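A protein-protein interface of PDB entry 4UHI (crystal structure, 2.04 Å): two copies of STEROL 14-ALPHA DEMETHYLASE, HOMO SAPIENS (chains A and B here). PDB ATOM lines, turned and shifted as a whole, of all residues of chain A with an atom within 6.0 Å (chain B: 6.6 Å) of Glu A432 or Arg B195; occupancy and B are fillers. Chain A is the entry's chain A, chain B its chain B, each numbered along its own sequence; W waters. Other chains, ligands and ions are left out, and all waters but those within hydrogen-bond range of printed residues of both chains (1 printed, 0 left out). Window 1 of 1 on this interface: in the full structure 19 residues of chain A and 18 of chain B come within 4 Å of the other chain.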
ATOM      1  N   TRP A 262      25.017  35.472  -4.047  1.00  0.00           N
ATOM      2  CA  TRP A 262      25.934  34.653  -3.276  1.00  0.00           C
ATOM      3  C   TRP A 262      26.249  35.317  -1.946  1.00  0.00           C
ATOM      4  O   TRP A 262      26.320  34.638  -0.909  1.00  0.00           O
ATOM      5  CB  TRP A 262      27.228  34.367  -4.040  1.00  0.00           C
ATOM      6  CG  TRP A 262      27.125  33.259  -5.060  1.00  0.00           C
ATOM      7  CD1 TRP A 262      27.245  33.378  -6.413  1.00  0.00           C
ATOM      8  CD2 TRP A 262      26.899  31.867  -4.801  1.00  0.00           C
ATOM      9  NE1 TRP A 262      27.120  32.155  -7.008  1.00  0.00           N
ATOM     10  CE2 TRP A 262      26.904  31.208  -6.043  1.00  0.00           C
ATOM     11  CE3 TRP A 262      26.695  31.116  -3.637  1.00  0.00           C
ATOM     12  CZ2 TRP A 262      26.705  29.837  -6.162  1.00  0.00           C
ATOM     13  CZ3 TRP A 262      26.518  29.732  -3.754  1.00  0.00           C
ATOM     14  CH2 TRP A 262      26.507  29.118  -5.006  1.00  0.00           C
ATOM     15  N   TYR A 418      19.884  24.986   4.475  1.00  0.00           N
ATOM     16  CA  TYR A 418      20.351  24.717   3.119  1.00  0.00           C
ATOM     17  C   TYR A 418      21.232  25.844   2.607  1.00  0.00           C
ATOM     18  O   TYR A 418      20.833  27.015   2.610  1.00  0.00           O
ATOM     19  CB  TYR A 418      19.167  24.542   2.170  1.00  0.00           C
ATOM     20  CG  TYR A 418      19.582  24.415   0.715  1.00  0.00           C
ATOM     21  CD1 TYR A 418      20.285  23.307   0.264  1.00  0.00           C
ATOM     22  CD2 TYR A 418      19.281  25.408  -0.194  1.00  0.00           C
ATOM     23  CE1 TYR A 418      20.666  23.198  -1.069  1.00  0.00           C
ATOM     24  CE2 TYR A 418      19.665  25.318  -1.513  1.00  0.00           C
ATOM     25  CZ  TYR A 418      20.351  24.217  -1.949  1.00  0.00           C
ATOM     26  OH  TYR A 418      20.705  24.153  -3.276  1.00  0.00           O
ATOM     27  N   PHE A 419      22.430  25.498   2.159  1.00  0.00           N
ATOM     28  CA  PHE A 419      23.288  26.471   1.486  1.00  0.00           C
ATOM     29  C   PHE A 419      23.370  26.115   0.020  1.00  0.00           C
ATOM     30  O   PHE A 419      23.820  25.030  -0.323  1.00  0.00           O
ATOM     31  CB  PHE A 419      24.692  26.498   2.106  1.00  0.00           C
ATOM     32  CG  PHE A 419      25.582  27.582   1.544  1.00  0.00           C
ATOM     33  CD1 PHE A 419      26.329  27.361   0.393  1.00  0.00           C
ATOM     34  CD2 PHE A 419      25.658  28.822   2.162  1.00  0.00           C
ATOM     35  CE1 PHE A 419      27.133  28.360  -0.128  1.00  0.00           C
ATOM     36  CE2 PHE A 419      26.468  29.828   1.652  1.00  0.00           C
ATOM     37  CZ  PHE A 419      27.201  29.596   0.505  1.00  0.00           C
ATOM     38  N   PRO A 420      22.957  27.038  -0.857  1.00  0.00           N
ATOM     39  CA  PRO A 420      22.881  26.716  -2.278  1.00  0.00           C
ATOM     40  C   PRO A 420      24.143  26.078  -2.861  1.00  0.00           C
ATOM     41  O   PRO A 420      25.260  26.522  -2.588  1.00  0.00           O
ATOM     42  CB  PRO A 420      22.632  28.079  -2.933  1.00  0.00           C
ATOM     43  CG  PRO A 420      21.896  28.863  -1.892  1.00  0.00           C
ATOM     44  CD  PRO A 420      22.473  28.404  -0.570  1.00  0.00           C
ATOM     45  N   THR A 421      23.946  25.058  -3.679  1.00  0.00           N
ATOM     46  CA  THR A 421      25.020  24.479  -4.468  1.00  0.00           C
ATOM     47  C   THR A 421      25.140  25.289  -5.743  1.00  0.00           C
ATOM     48  O   THR A 421      24.246  26.052  -6.082  1.00  0.00           O
ATOM     49  CB  THR A 421      24.717  23.007  -4.836  1.00  0.00           C
ATOM     50  OG1 THR A 421      23.386  22.912  -5.335  1.00  0.00           O
ATOM     51  CG2 THR A 421      24.849  22.089  -3.614  1.00  0.00           C
ATOM     52  N   VAL A 422      26.259  25.138  -6.440  1.00  0.00           N
ATOM     53  CA  VAL A 422      26.512  25.903  -7.664  1.00  0.00           C
ATOM     54  C   VAL A 422      25.827  25.230  -8.854  1.00  0.00           C
ATOM     55  O   VAL A 422      25.989  24.038  -9.079  1.00  0.00           O
ATOM     56  CB  VAL A 422      28.035  26.037  -7.966  1.00  0.00           C
ATOM     57  CG1 VAL A 422      28.266  26.886  -9.205  1.00  0.00           C
ATOM     58  CG2 VAL A 422      28.784  26.640  -6.787  1.00  0.00           C
ATOM     59  N   ASN A 423      25.070  26.012  -9.618  1.00  0.00           N
ATOM     60  CA  ASN A 423      24.489  25.544 -10.848  1.00  0.00           C
ATOM     61  C   ASN A 423      25.427  25.743 -12.037  1.00  0.00           C
ATOM     62  O   ASN A 423      25.459  26.812 -12.626  1.00  0.00           O
ATOM     63  CB  ASN A 423      23.168  26.264 -11.127  1.00  0.00           C
ATOM     64  CG  ASN A 423      22.452  25.715 -12.364  1.00  0.00           C
ATOM     65  OD1 ASN A 423      22.993  24.886 -13.100  1.00  0.00           O
ATOM     66  ND2 ASN A 423      21.230  26.176 -12.591  1.00  0.00           N
ATOM     67  N   TYR A 424      26.139  24.681 -12.413  1.00  0.00           N
ATOM     68  CA  TYR A 424      27.065  24.708 -13.537  1.00  0.00           C
ATOM     69  C   TYR A 424      26.409  24.591 -14.925  1.00  0.00           C
ATOM     70  O   TYR A 424      27.108  24.538 -15.920  1.00  0.00           O
ATOM     71  CB  TYR A 424      28.087  23.592 -13.377  1.00  0.00           C
ATOM     72  CG  TYR A 424      28.985  23.790 -12.189  1.00  0.00           C
ATOM     73  CD1 TYR A 424      29.985  24.753 -12.212  1.00  0.00           C
ATOM     74  CD2 TYR A 424      28.823  23.038 -11.037  1.00  0.00           C
ATOM     75  CE1 TYR A 424      30.806  24.956 -11.129  1.00  0.00           C
ATOM     76  CE2 TYR A 424      29.650  23.229  -9.941  1.00  0.00           C
ATOM     77  CZ  TYR A 424      30.642  24.192 -10.000  1.00  0.00           C
ATOM     78  OH  TYR A 424      31.463  24.422  -8.925  1.00  0.00           O
ATOM     79  N   THR A 425      25.078  24.566 -14.998  1.00  0.00           N
ATOM     80  CA  THR A 425      24.405  24.464 -16.290  1.00  0.00           C
ATOM     81  C   THR A 425      24.100  25.824 -16.924  1.00  0.00           C
ATOM     82  O   THR A 425      23.712  25.883 -18.086  1.00  0.00           O
ATOM     83  CB  THR A 425      23.100  23.670 -16.187  1.00  0.00           C
ATOM     84  OG1 THR A 425      22.130  24.430 -15.465  1.00  0.00           O
ATOM     85  CG2 THR A 425      23.336  22.330 -15.486  1.00  0.00           C
ATOM     86  N   THR A 430      25.165  30.083 -11.200  1.00  0.00           N
ATOM     87  CA  THR A 430      24.154  30.634 -10.314  1.00  0.00           C
ATOM     88  C   THR A 430      24.012  29.730  -9.100  1.00  0.00           C
ATOM     89  O   THR A 430      24.247  28.539  -9.202  1.00  0.00           O
ATOM     90  CB  THR A 430      22.811  30.642 -11.028  1.00  0.00           C
ATOM     91  OG1 THR A 430      22.596  29.351 -11.600  1.00  0.00           O
ATOM     92  CG2 THR A 430      22.807  31.682 -12.131  1.00  0.00           C
ATOM     93  N   PRO A 431      23.589  30.287  -7.954  1.00  0.00           N
ATOM     94  CA  PRO A 431      23.269  29.430  -6.810  1.00  0.00           C
ATOM     95  C   PRO A 431      22.001  28.607  -7.082  1.00  0.00           C
ATOM     96  O   PRO A 431      21.048  29.146  -7.602  1.00  0.00           O
ATOM     97  CB  PRO A 431      23.023  30.427  -5.683  1.00  0.00           C
ATOM     98  CG  PRO A 431      22.598  31.671  -6.357  1.00  0.00           C
ATOM     99  CD  PRO A 431      23.108  31.657  -7.772  1.00  0.00           C
ATOM    100  N   GLU A 432      22.015  27.316  -6.750  1.00  0.00           N
ATOM    101  CA  GLU A 432      20.844  26.449  -6.932  1.00  0.00           C
ATOM    102  C   GLU A 432      19.794  26.751  -5.875  1.00  0.00           C
ATOM    103  O   GLU A 432      20.126  26.988  -4.711  1.00  0.00           O
ATOM    104  CB  GLU A 432      21.232  24.966  -6.825  1.00  0.00           C
ATOM    105  CG  GLU A 432      21.836  24.372  -8.091  1.00  0.00           C
ATOM    106  CD  GLU A 432      20.800  24.078  -9.165  1.00  0.00           C
ATOM    107  OE1 GLU A 432      19.589  24.100  -8.852  1.00  0.00           O
ATOM    108  OE2 GLU A 432      21.204  23.830 -10.327  1.00  0.00           O
ATOM    109  N   ASN A 433      18.531  26.724  -6.278  1.00  0.00           N
ATOM    110  CA  ASN A 433      17.415  26.978  -5.358  1.00  0.00           C
ATOM    111  C   ASN A 433      17.685  28.189  -4.436  1.00  0.00           C
ATOM    112  O   ASN A 433      17.721  28.049  -3.221  1.00  0.00           O
ATOM    113  CB  ASN A 433      17.137  25.711  -4.544  1.00  0.00           C
ATOM    114  CG  ASN A 433      15.940  25.844  -3.601  1.00  0.00           C
ATOM    115  OD1 ASN A 433      15.858  25.133  -2.601  1.00  0.00           O
ATOM    116  ND2 ASN A 433      15.018  26.731  -3.915  1.00  0.00           N
ATOM    117  N   PRO A 434      17.870  29.389  -5.026  1.00  0.00           N
ATOM    118  CA  PRO A 434      18.296  30.551  -4.241  1.00  0.00           C
ATOM    119  C   PRO A 434      17.152  31.272  -3.508  1.00  0.00           C
ATOM    120  O   PRO A 434      17.040  32.505  -3.573  1.00  0.00           O
ATOM    121  CB  PRO A 434      18.906  31.461  -5.303  1.00  0.00           C
ATOM    122  CG  PRO A 434      18.083  31.204  -6.510  1.00  0.00           C
ATOM    123  CD  PRO A 434      17.768  29.716  -6.462  1.00  0.00           C
ATOM    124  N   VAL A 435      16.330  30.510  -2.800  1.00  0.00           N
ATOM    125  CA  VAL A 435      15.257  31.086  -1.999  1.00  0.00           C
ATOM    126  C   VAL A 435      15.781  31.336  -0.607  1.00  0.00           C
ATOM    127  O   VAL A 435      16.392  30.457   0.006  1.00  0.00           O
ATOM    128  CB  VAL A 435      14.016  30.174  -1.934  1.00  0.00           C
ATOM    129  CG1 VAL A 435      12.919  30.812  -1.077  1.00  0.00           C
ATOM    130  CG2 VAL A 435      13.500  29.893  -3.344  1.00  0.00           C
ATOM    131  N   LYS B 162      10.702  25.843  -6.694  1.00  0.00           N
ATOM    132  CA  LYS B 162      11.745  24.933  -7.115  1.00  0.00           C
ATOM    133  C   LYS B 162      11.181  23.850  -8.024  1.00  0.00           C
ATOM    134  O   LYS B 162      11.772  23.520  -9.049  1.00  0.00           O
ATOM    135  CB  LYS B 162      12.426  24.280  -5.910  1.00  0.00           C
ATOM    136  CG  LYS B 162      13.497  23.278  -6.302  1.00  0.00           C
ATOM    137  CD  LYS B 162      13.839  22.315  -5.184  1.00  0.00           C
ATOM    138  CE  LYS B 162      15.011  21.431  -5.597  1.00  0.00           C
ATOM    139  NZ  LYS B 162      15.692  20.805  -4.433  1.00  0.00           N
ATOM    140  N   LEU B 166      11.573  22.669 -12.125  1.00  0.00           N
ATOM    141  CA  LEU B 166      11.843  21.345 -12.660  1.00  0.00           C
ATOM    142  C   LEU B 166      10.942  21.064 -13.863  1.00  0.00           C
ATOM    143  O   LEU B 166      11.384  20.498 -14.857  1.00  0.00           O
ATOM    144  CB  LEU B 166      11.663  20.276 -11.585  1.00  0.00           C
ATOM    145  CG  LEU B 166      12.606  20.387 -10.384  1.00  0.00           C
ATOM    146  CD1 LEU B 166      12.319  19.294  -9.356  1.00  0.00           C
ATOM    147  CD2 LEU B 166      14.076  20.336 -10.824  1.00  0.00           C
ATOM    148  N   ASP B 169      12.261  22.890 -16.784  1.00  0.00           N
ATOM    149  CA  ASP B 169      13.394  22.125 -17.288  1.00  0.00           C
ATOM    150  C   ASP B 169      12.888  21.021 -18.214  1.00  0.00           C
ATOM    151  O   ASP B 169      13.501  20.731 -19.254  1.00  0.00           O
ATOM    152  CB  ASP B 169      14.210  21.499 -16.136  1.00  0.00           C
ATOM    153  CG  ASP B 169      14.882  22.550 -15.215  1.00  0.00           C
ATOM    154  OD1 ASP B 169      15.038  23.726 -15.620  1.00  0.00           O
ATOM    155  OD2 ASP B 169      15.256  22.178 -14.074  1.00  0.00           O
ATOM    156  N   PHE B 190      19.725  19.368 -22.028  1.00  0.00           N
ATOM    157  CA  PHE B 190      19.649  17.918 -21.878  1.00  0.00           C
ATOM    158  C   PHE B 190      19.900  17.507 -20.431  1.00  0.00           C
ATOM    159  O   PHE B 190      19.247  16.603 -19.910  1.00  0.00           O
ATOM    160  CB  PHE B 190      20.698  17.225 -22.757  1.00  0.00           C
ATOM    161  CG  PHE B 190      20.444  17.332 -24.241  1.00  0.00           C
ATOM    162  CD1 PHE B 190      19.491  18.210 -24.757  1.00  0.00           C
ATOM    163  CD2 PHE B 190      21.196  16.567 -25.132  1.00  0.00           C
ATOM    164  CE1 PHE B 190      19.287  18.308 -26.130  1.00  0.00           C
ATOM    165  CE2 PHE B 190      20.993  16.662 -26.503  1.00  0.00           C
ATOM    166  CZ  PHE B 190      20.043  17.539 -27.002  1.00  0.00           C
ATOM    167  N   ARG B 191      20.886  18.142 -19.807  1.00  0.00           N
ATOM    168  CA  ARG B 191      21.252  17.824 -18.441  1.00  0.00           C
ATOM    169  C   ARG B 191      20.172  18.280 -17.460  1.00  0.00           C
ATOM    170  O   ARG B 191      19.831  17.555 -16.541  1.00  0.00           O
ATOM    171  CB  ARG B 191      22.578  18.487 -18.076  1.00  0.00           C
ATOM    172  CG  ARG B 191      23.774  17.971 -18.857  1.00  0.00           C
ATOM    173  CD  ARG B 191      24.948  18.940 -18.741  1.00  0.00           C
ATOM    174  NE  ARG B 191      25.372  19.127 -17.352  1.00  0.00           N
ATOM    175  CZ  ARG B 191      26.185  20.097 -16.934  1.00  0.00           C
ATOM    176  NH1 ARG B 191      26.673  20.979 -17.798  1.00  0.00           N
ATOM    177  NH2 ARG B 191      26.513  20.183 -15.650  1.00  0.00           N
ATOM    178  N   ARG B 192      19.665  19.496 -17.645  1.00  0.00           N
ATOM    179  CA  ARG B 192      18.605  20.024 -16.782  1.00  0.00           C
ATOM    180  C   ARG B 192      17.321  19.192 -16.931  1.00  0.00           C
ATOM    181  O   ARG B 192      16.646  18.900 -15.946  1.00  0.00           O
ATOM    182  CB  ARG B 192      18.342  21.501 -17.088  1.00  0.00           C
ATOM    183  CG  ARG B 192      19.425  22.453 -16.569  1.00  0.00           C
ATOM    184  CD  ARG B 192      19.008  23.902 -16.749  1.00  0.00           C
ATOM    185  NE  ARG B 192      18.874  24.238 -18.163  1.00  0.00           N
ATOM    186  CZ  ARG B 192      19.564  25.184 -18.804  1.00  0.00           C
ATOM    187  NH1 ARG B 192      20.441  25.963 -18.156  1.00  0.00           N
ATOM    188  NH2 ARG B 192      19.353  25.370 -20.107  1.00  0.00           N
ATOM    189  N   ARG B 193      17.015  18.787 -18.161  1.00  0.00           N
ATOM    190  CA  ARG B 193      15.865  17.893 -18.430  1.00  0.00           C
ATOM    191  C   ARG B 193      15.945  16.593 -17.639  1.00  0.00           C
ATOM    192  O   ARG B 193      15.004  16.221 -16.934  1.00  0.00           O
ATOM    193  CB  ARG B 193      15.773  17.569 -19.922  1.00  0.00           C
ATOM    194  CG  ARG B 193      14.653  16.602 -20.279  1.00  0.00           C
ATOM    195  CD  ARG B 193      14.854  16.007 -21.656  1.00  0.00           C
ATOM    196  NE  ARG B 193      16.106  15.278 -21.703  1.00  0.00           N
ATOM    197  CZ  ARG B 193      16.835  15.081 -22.800  1.00  0.00           C
ATOM    198  NH1 ARG B 193      16.429  15.526 -23.983  1.00  0.00           N
ATOM    199  NH2 ARG B 193      17.972  14.415 -22.705  1.00  0.00           N
ATOM    200  N   ASP B 194      17.073  15.900 -17.764  1.00  0.00           N
ATOM    201  CA  ASP B 194      17.248  14.586 -17.141  1.00  0.00           C
ATOM    202  C   ASP B 194      17.294  14.650 -15.615  1.00  0.00           C
ATOM    203  O   ASP B 194      16.849  13.733 -14.947  1.00  0.00           O
ATOM    204  CB  ASP B 194      18.518  13.925 -17.653  1.00  0.00           C
ATOM    205  CG  ASP B 194      18.500  13.707 -19.150  1.00  0.00           C
ATOM    206  OD1 ASP B 194      17.402  13.733 -19.750  1.00  0.00           O
ATOM    207  OD2 ASP B 194      19.588  13.510 -19.729  1.00  0.00           O
ATOM    208  N   ARG B 195      17.875  15.723 -15.081  1.00  0.00           N
ATOM    209  CA  ARG B 195      17.880  15.982 -13.642  1.00  0.00           C
ATOM    210  C   ARG B 195      16.457  16.246 -13.148  1.00  0.00           C
ATOM    211  O   ARG B 195      16.053  15.769 -12.091  1.00  0.00           O
ATOM    212  CB  ARG B 195      18.768  17.194 -13.340  1.00  0.00           C
ATOM    213  CG  ARG B 195      18.812  17.626 -11.877  1.00  0.00           C
ATOM    214  CD  ARG B 195      19.545  18.957 -11.724  1.00  0.00           C
ATOM    215  NE  ARG B 195      19.551  19.442 -10.339  1.00  0.00           N
ATOM    216  CZ  ARG B 195      18.650  20.282  -9.821  1.00  0.00           C
ATOM    217  NH1 ARG B 195      17.652  20.749 -10.565  1.00  0.00           N
ATOM    218  NH2 ARG B 195      18.743  20.655  -8.548  1.00  0.00           N
ATOM    219  N   ALA B 196      15.716  17.043 -13.903  1.00  0.00           N
ATOM    220  CA  ALA B 196      14.366  17.399 -13.525  1.00  0.00           C
ATOM    221  C   ALA B 196      13.492  16.147 -13.532  1.00  0.00           C
ATOM    222  O   ALA B 196      12.680  15.942 -12.627  1.00  0.00           O
ATOM    223  CB  ALA B 196      13.818  18.438 -14.472  1.00  0.00           C
ATOM    224  N   HIS B 197      13.702  15.300 -14.537  1.00  0.00           N
ATOM    225  CA  HIS B 197      12.955  14.053 -14.680  1.00  0.00           C
ATOM    226  C   HIS B 197      13.150  13.150 -13.475  1.00  0.00           C
ATOM    227  O   HIS B 197      12.180  12.567 -12.959  1.00  0.00           O
ATOM    228  CB  HIS B 197      13.386  13.312 -15.953  1.00  0.00           C
ATOM    229  CG  HIS B 197      12.557  12.106 -16.259  1.00  0.00           C
ATOM    230  ND1 HIS B 197      11.365  12.178 -16.948  1.00  0.00           N
ATOM    231  CD2 HIS B 197      12.743  10.799 -15.963  1.00  0.00           C
ATOM    232  CE1 HIS B 197      10.850  10.966 -17.061  1.00  0.00           C
ATOM    233  NE2 HIS B 197      11.666  10.111 -16.472  1.00  0.00           N
ATOM    234  N   ARG B 198      14.408  13.025 -13.039  1.00  0.00           N
ATOM    235  CA  ARG B 198      14.749  12.181 -11.896  1.00  0.00           C
ATOM    236  C   ARG B 198      14.124  12.730 -10.621  1.00  0.00           C
ATOM    237  O   ARG B 198      13.509  11.994  -9.859  1.00  0.00           O
ATOM    238  CB  ARG B 198      16.267  12.085 -11.721  1.00  0.00           C
ATOM    239  CG  ARG B 198      16.980  11.253 -12.773  1.00  0.00           C
ATOM    240  CD  ARG B 198      18.454  11.044 -12.417  1.00  0.00           C
ATOM    241  NE  ARG B 198      19.215  12.301 -12.387  1.00  0.00           N
ATOM    242  CZ  ARG B 198      19.847  12.835 -13.437  1.00  0.00           C
ATOM    243  NH1 ARG B 198      19.829  12.228 -14.620  1.00  0.00           N
ATOM    244  NH2 ARG B 198      20.501  13.984 -13.303  1.00  0.00           N
ATOM    245  N   GLU B 199      14.283  14.030 -10.402  1.00  0.00           N
ATOM    246  CA  GLU B 199      13.769  14.675  -9.203  1.00  0.00           C
ATOM    247  C   GLU B 199      12.230  14.670  -9.117  1.00  0.00           C
ATOM    248  O   GLU B 199      11.671  14.473  -8.032  1.00  0.00           O
ATOM    249  CB  GLU B 199      14.299  16.103  -9.096  1.00  0.00           C
ATOM    250  CG  GLU B 199      15.787  16.167  -8.792  1.00  0.00           C
ATOM    251  CD  GLU B 199      16.192  17.435  -8.071  1.00  0.00           C
ATOM    252  OE1 GLU B 199      15.617  17.736  -7.003  1.00  0.00           O
ATOM    253  OE2 GLU B 199      17.103  18.123  -8.564  1.00  0.00           O
ATOM    254  N   ILE B 200      11.556  14.898 -10.247  1.00  0.00           N
ATOM    255  CA  ILE B 200      10.085  14.853 -10.290  1.00  0.00           C
ATOM    256  C   ILE B 200       9.576  13.437 -10.067  1.00  0.00           C
ATOM    257  O   ILE B 200       8.624  13.235  -9.321  1.00  0.00           O
ATOM    258  CB  ILE B 200       9.524  15.389 -11.621  1.00  0.00           C
ATOM    259  CG1 ILE B 200       9.553  16.913 -11.619  1.00  0.00           C
ATOM    260  CG2 ILE B 200       8.091  14.925 -11.822  1.00  0.00           C
ATOM    261  CD1 ILE B 200       9.325  17.527 -12.983  1.00  0.00           C
HETATM  262  O   HOH W   1      16.992  22.397  -2.191  1.00  0.00           O
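OH of Tyr A418 is in hydrogen-bond range of O of Glu A432 (3.2 Å). The backbone NH (N) of Glu A432 is in hydrogen-bond range of the backbone carbonyl oxygen (O) of Thr A421 (2.6 Å). The side-chain hydroxyl of Thr A425 lies within hydrogen-bond range of the side-chain amide oxygen of Asn A423. The side-chain carboxylate (OE2) of Glu A432 sits close to the side-chain amide nitrogen (ND2) of Asn A423. OE2 of Glu B199 lies within salt-bridge range of NH2 of Arg B195 (3.0 Å).
Water W1 bridges the side-chain amide oxygen (OD1) of Asn A433 (3.0 Å) and the side-chain amino group (NZ) of Lys B162 (3.0 Å).
Of the printed residues of chain B, Glu A432 touches Arg B195. Of chain A, only Glu A432 (3.6 Å) comes within 4 Å of Arg B195. Of the printed residues of chain A, Arg B191 touches Thr A425 (3.8 Å). Of the printed residues of chain B, Thr A425 touches Arg B191 and Arg B192. Trp A262 touches none of the printed residues of chain B. Pro A431 touches none of the printed residues of chain B. The nearest residue of chain B that does not touch Glu A432 is Lys B162 (6.2 Å).
No position is printed for both chains. Of the 3 pairs that touch across the chains among the printed residues, none has its exchanged pair printed and touching as well.
Thr A425 touches Arg B191 (CG2 to NH2, 3.8 Å).
Of the 15 printed residues of chain A, 2 touch a printed residue of chain B. Printed residues of chain A that touch a printed residue of chain B: Thr A425 and Glu A432. Printed residues of chain B that touch a printed residue of chain A: Arg B191, Arg B192 and Arg B195. Among the printed residues, 3 pairs touch across the chains.
The guanidinium group of Arg B192 lies within hydrogen-bond range of the backbone carbonyl oxygen of Thr A425 (3.3 Å). The side-chain carboxylate (OE1) of Glu A432 lies within salt-bridge range of the guanidinium group (NH2) of Arg B195.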
